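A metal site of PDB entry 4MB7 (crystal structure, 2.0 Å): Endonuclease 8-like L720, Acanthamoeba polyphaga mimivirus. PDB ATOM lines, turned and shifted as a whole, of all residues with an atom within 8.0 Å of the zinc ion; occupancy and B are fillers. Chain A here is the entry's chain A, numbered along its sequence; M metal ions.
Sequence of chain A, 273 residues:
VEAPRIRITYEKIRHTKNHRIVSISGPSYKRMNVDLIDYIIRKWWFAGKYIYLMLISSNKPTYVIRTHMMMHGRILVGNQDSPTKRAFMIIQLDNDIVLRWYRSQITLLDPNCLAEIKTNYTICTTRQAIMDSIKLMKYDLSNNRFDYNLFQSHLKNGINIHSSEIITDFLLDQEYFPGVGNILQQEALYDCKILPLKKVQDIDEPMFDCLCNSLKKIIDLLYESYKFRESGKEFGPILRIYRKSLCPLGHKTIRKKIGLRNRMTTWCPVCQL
The backbone NH of Leu 249 lies close to the side-chain sulfur of Cys 247 (3.2 Å). SG of Cys 247 lies close to N of Gly 250, at 3.5 Å. The backbone NH (N) of Val 270 lies close to the side-chain sulfur (SG) of Cys 268 (3.5 Å). The backbone NH of Cys 268 is in hydrogen-bond range of the side-chain amide oxygen of Gln 272 (2.8 Å). O of Cys 271 sits at hydrogen-bond distance from NZ of Lys 193, at 2.8 Å.
Of the 17 residues printed, 4 come within 4 Å of the zinc ion.
The zinc ion is bound by ND1 of His 251 (2.0 Å), SG of Cys 247 (2.2 Å), SG of Cys 268 (2.3 Å) and SG of Cys 271 (2.3 Å).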
ATOM      1  N   TYR A 190      -9.994  14.708 -31.467  1.00  0.00           N
ATOM      2  CA  TYR A 190      -8.934  15.433 -30.779  1.00  0.00           C
ATOM      3  C   TYR A 190      -7.611  14.683 -30.877  1.00  0.00           C
ATOM      4  O   TYR A 190      -6.559  15.292 -31.056  1.00  0.00           O
ATOM      5  CB  TYR A 190      -9.264  15.673 -29.307  1.00  0.00           C
ATOM      6  CG  TYR A 190      -8.099  16.296 -28.570  1.00  0.00           C
ATOM      7  CD1 TYR A 190      -7.785  17.634 -28.747  1.00  0.00           C
ATOM      8  CD2 TYR A 190      -7.300  15.531 -27.726  1.00  0.00           C
ATOM      9  CE1 TYR A 190      -6.707  18.203 -28.092  1.00  0.00           C
ATOM     10  CE2 TYR A 190      -6.215  16.094 -27.072  1.00  0.00           C
ATOM     11  CZ  TYR A 190      -5.926  17.437 -27.262  1.00  0.00           C
ATOM     12  OH  TYR A 190      -4.860  18.010 -26.613  1.00  0.00           O
ATOM     13  N   LYS A 193      -6.188  15.427 -34.125  1.00  0.00           N
ATOM     14  CA  LYS A 193      -6.075  16.856 -34.423  1.00  0.00           C
ATOM     15  C   LYS A 193      -6.924  17.284 -35.621  1.00  0.00           C
ATOM     16  O   LYS A 193      -6.488  18.075 -36.451  1.00  0.00           O
ATOM     17  CB  LYS A 193      -4.607  17.253 -34.642  1.00  0.00           C
ATOM     18  CG  LYS A 193      -3.758  17.171 -33.384  1.00  0.00           C
ATOM     19  CD  LYS A 193      -2.269  17.219 -33.708  1.00  0.00           C
ATOM     20  CE  LYS A 193      -1.896  18.475 -34.471  1.00  0.00           C
ATOM     21  NZ  LYS A 193      -2.188  19.721 -33.691  1.00  0.00           N
ATOM     22  N   ILE A 241     -10.684  15.130 -23.905  1.00  0.00           N
ATOM     23  CA  ILE A 241     -11.365  16.324 -24.407  1.00  0.00           C
ATOM     24  C   ILE A 241     -12.846  16.371 -24.034  1.00  0.00           C
ATOM     25  O   ILE A 241     -13.479  17.424 -24.102  1.00  0.00           O
ATOM     26  CB  ILE A 241     -11.211  16.451 -25.946  1.00  0.00           C
ATOM     27  CG1 ILE A 241     -11.385  17.910 -26.382  1.00  0.00           C
ATOM     28  CG2 ILE A 241     -12.190  15.533 -26.668  1.00  0.00           C
ATOM     29  CD1 ILE A 241     -10.343  18.841 -25.820  1.00  0.00           C
ATOM     30  N   LEU A 246     -10.313  22.862 -20.487  1.00  0.00           N
ATOM     31  CA  LEU A 246      -8.975  23.051 -21.045  1.00  0.00           C
ATOM     32  C   LEU A 246      -8.436  21.748 -21.649  1.00  0.00           C
ATOM     33  O   LEU A 246      -8.473  20.709 -21.009  1.00  0.00           O
ATOM     34  CB  LEU A 246      -8.015  23.534 -19.968  1.00  0.00           C
ATOM     35  CG  LEU A 246      -7.954  25.039 -19.694  1.00  0.00           C
ATOM     36  CD1 LEU A 246      -7.629  25.830 -20.950  1.00  0.00           C
ATOM     37  CD2 LEU A 246      -9.283  25.497 -19.112  1.00  0.00           C
ATOM     38  N   CYS A 247      -7.917  21.837 -22.862  1.00  0.00           N
ATOM     39  CA  CYS A 247      -7.272  20.690 -23.492  1.00  0.00           C
ATOM     40  C   CYS A 247      -6.024  20.356 -22.680  1.00  0.00           C
ATOM     41  O   CYS A 247      -5.526  21.213 -21.939  1.00  0.00           O
ATOM     42  CB  CYS A 247      -6.926  20.996 -24.954  1.00  0.00           C
ATOM     43  SG  CYS A 247      -5.316  21.761 -25.215  1.00  0.00           S
ATOM     44  N   PRO A 248      -5.514  19.121 -22.800  1.00  0.00           N
ATOM     45  CA  PRO A 248      -4.353  18.746 -21.978  1.00  0.00           C
ATOM     46  C   PRO A 248      -3.084  19.568 -22.251  1.00  0.00           C
ATOM     47  O   PRO A 248      -2.133  19.472 -21.484  1.00  0.00           O
ATOM     48  CB  PRO A 248      -4.118  17.265 -22.336  1.00  0.00           C
ATOM     49  CG  PRO A 248      -4.843  17.055 -23.618  1.00  0.00           C
ATOM     50  CD  PRO A 248      -6.012  17.983 -23.583  1.00  0.00           C
ATOM     51  N   LEU A 249      -3.079  20.353 -23.325  1.00  0.00           N
ATOM     52  CA  LEU A 249      -1.966  21.261 -23.580  1.00  0.00           C
ATOM     53  C   LEU A 249      -2.169  22.597 -22.858  1.00  0.00           C
ATOM     54  O   LEU A 249      -1.209  23.321 -22.617  1.00  0.00           O
ATOM     55  CB  LEU A 249      -1.777  21.498 -25.085  1.00  0.00           C
ATOM     56  CG  LEU A 249      -1.187  20.324 -25.883  1.00  0.00           C
ATOM     57  CD1 LEU A 249      -0.894  20.741 -27.312  1.00  0.00           C
ATOM     58  CD2 LEU A 249       0.072  19.799 -25.192  1.00  0.00           C
ATOM     59  N   GLY A 250      -3.419  22.905 -22.534  1.00  0.00           N
ATOM     60  CA  GLY A 250      -3.735  24.104 -21.777  1.00  0.00           C
ATOM     61  C   GLY A 250      -4.578  25.127 -22.514  1.00  0.00           C
ATOM     62  O   GLY A 250      -4.832  26.213 -21.997  1.00  0.00           O
ATOM     63  N   HIS A 251      -5.011  24.778 -23.721  1.00  0.00           N
ATOM     64  CA  HIS A 251      -5.827  25.698 -24.517  1.00  0.00           C
ATOM     65  C   HIS A 251      -7.271  25.696 -24.044  1.00  0.00           C
ATOM     66  O   HIS A 251      -7.765  24.704 -23.515  1.00  0.00           O
ATOM     67  CB  HIS A 251      -5.781  25.307 -25.992  1.00  0.00           C
ATOM     68  CG  HIS A 251      -4.396  25.069 -26.513  1.00  0.00           C
ATOM     69  ND1 HIS A 251      -4.096  24.033 -27.371  1.00  0.00           N
ATOM     70  CD2 HIS A 251      -3.231  25.727 -26.300  1.00  0.00           C
ATOM     71  CE1 HIS A 251      -2.812  24.054 -27.667  1.00  0.00           C
ATOM     72  NE2 HIS A 251      -2.262  25.083 -27.031  1.00  0.00           N
ATOM     73  N   LYS A 252      -7.952  26.820 -24.245  1.00  0.00           N
ATOM     74  CA  LYS A 252      -9.368  26.922 -23.930  1.00  0.00           C
ATOM     75  C   LYS A 252     -10.183  26.249 -25.039  1.00  0.00           C
ATOM     76  O   LYS A 252      -9.942  26.474 -26.222  1.00  0.00           O
ATOM     77  CB  LYS A 252      -9.784  28.390 -23.786  1.00  0.00           C
ATOM     78  CG  LYS A 252     -11.252  28.590 -23.446  1.00  0.00           C
ATOM     79  N   THR A 253     -11.146  25.432 -24.647  1.00  0.00           N
ATOM     80  CA  THR A 253     -11.925  24.648 -25.603  1.00  0.00           C
ATOM     81  C   THR A 253     -13.245  25.305 -25.981  1.00  0.00           C
ATOM     82  O   THR A 253     -13.703  26.239 -25.332  1.00  0.00           O
ATOM     83  CB  THR A 253     -12.217  23.237 -25.056  1.00  0.00           C
ATOM     84  OG1 THR A 253     -13.062  23.335 -23.904  1.00  0.00           O
ATOM     85  CG2 THR A 253     -10.925  22.527 -24.680  1.00  0.00           C
ATOM     86  N   TRP A 267     -14.164  20.633 -28.634  1.00  0.00           N
ATOM     87  CA  TRP A 267     -12.934  20.550 -29.424  1.00  0.00           C
ATOM     88  C   TRP A 267     -12.006  21.717 -29.141  1.00  0.00           C
ATOM     89  O   TRP A 267     -12.444  22.783 -28.718  1.00  0.00           O
ATOM     90  CB  TRP A 267     -13.254  20.483 -30.925  1.00  0.00           C
ATOM     91  CG  TRP A 267     -13.676  21.791 -31.525  1.00  0.00           C
ATOM     92  CD1 TRP A 267     -12.863  22.760 -32.030  1.00  0.00           C
ATOM     93  CD2 TRP A 267     -15.018  22.266 -31.715  1.00  0.00           C
ATOM     94  NE1 TRP A 267     -13.612  23.819 -32.508  1.00  0.00           N
ATOM     95  CE2 TRP A 267     -14.939  23.531 -32.327  1.00  0.00           C
ATOM     96  CE3 TRP A 267     -16.283  21.744 -31.413  1.00  0.00           C
ATOM     97  CZ2 TRP A 267     -16.069  24.285 -32.649  1.00  0.00           C
ATOM     98  CZ3 TRP A 267     -17.406  22.491 -31.736  1.00  0.00           C
ATOM     99  CH2 TRP A 267     -17.284  23.741 -32.346  1.00  0.00           C
ATOM    100  N   CYS A 268     -10.715  21.502 -29.369  1.00  0.00           N
ATOM    101  CA  CYS A 268      -9.728  22.551 -29.221  1.00  0.00           C
ATOM    102  C   CYS A 268      -9.463  23.217 -30.566  1.00  0.00           C
ATOM    103  O   CYS A 268      -8.996  22.563 -31.494  1.00  0.00           O
ATOM    104  CB  CYS A 268      -8.431  21.994 -28.642  1.00  0.00           C
ATOM    105  SG  CYS A 268      -7.107  23.208 -28.529  1.00  0.00           S
ATOM    106  N   PRO A 269      -9.758  24.519 -30.677  1.00  0.00           N
ATOM    107  CA  PRO A 269      -9.606  25.259 -31.930  1.00  0.00           C
ATOM    108  C   PRO A 269      -8.141  25.394 -32.346  1.00  0.00           C
ATOM    109  O   PRO A 269      -7.847  25.625 -33.518  1.00  0.00           O
ATOM    110  CB  PRO A 269     -10.197  26.635 -31.602  1.00  0.00           C
ATOM    111  CG  PRO A 269     -10.022  26.765 -30.134  1.00  0.00           C
ATOM    112  CD  PRO A 269     -10.235  25.385 -29.583  1.00  0.00           C
ATOM    113  N   VAL A 270      -7.247  25.259 -31.379  1.00  0.00           N
ATOM    114  CA  VAL A 270      -5.810  25.333 -31.647  1.00  0.00           C
ATOM    115  C   VAL A 270      -5.258  23.977 -32.085  1.00  0.00           C
ATOM    116  O   VAL A 270      -4.697  23.855 -33.175  1.00  0.00           O
ATOM    117  CB  VAL A 270      -5.031  25.817 -30.407  1.00  0.00           C
ATOM    118  CG1 VAL A 270      -3.533  25.826 -30.684  1.00  0.00           C
ATOM    119  CG2 VAL A 270      -5.507  27.207 -30.008  1.00  0.00           C
ATOM    120  N   CYS A 271      -5.431  22.962 -31.249  1.00  0.00           N
ATOM    121  CA  CYS A 271      -4.920  21.630 -31.539  1.00  0.00           C
ATOM    122  C   CYS A 271      -5.575  21.012 -32.770  1.00  0.00           C
ATOM    123  O   CYS A 271      -4.909  20.404 -33.604  1.00  0.00           O
ATOM    124  CB  CYS A 271      -5.113  20.695 -30.333  1.00  0.00           C
ATOM    125  SG  CYS A 271      -4.133  21.130 -28.884  1.00  0.00           S
ATOM    126  N   GLN A 272      -6.884  21.191 -32.878  1.00  0.00           N
ATOM    127  CA  GLN A 272      -7.642  20.624 -33.983  1.00  0.00           C
ATOM    128  C   GLN A 272      -7.922  21.678 -35.045  1.00  0.00           C
ATOM    129  O   GLN A 272      -8.739  22.578 -34.840  1.00  0.00           O
ATOM    130  CB  GLN A 272      -8.960  20.025 -33.477  1.00  0.00           C
ATOM    131  CG  GLN A 272      -8.765  18.937 -32.440  1.00  0.00           C
ATOM    132  CD  GLN A 272     -10.054  18.604 -31.703  1.00  0.00           C
ATOM    133  OE1 GLN A 272     -10.228  18.963 -30.548  1.00  0.00           O
ATOM    134  NE2 GLN A 272     -10.960  17.909 -32.380  1.00  0.00           N
HETATM  135 ZN    ZN M   1      -5.342  22.422 -27.348  1.00  0.00          ZN
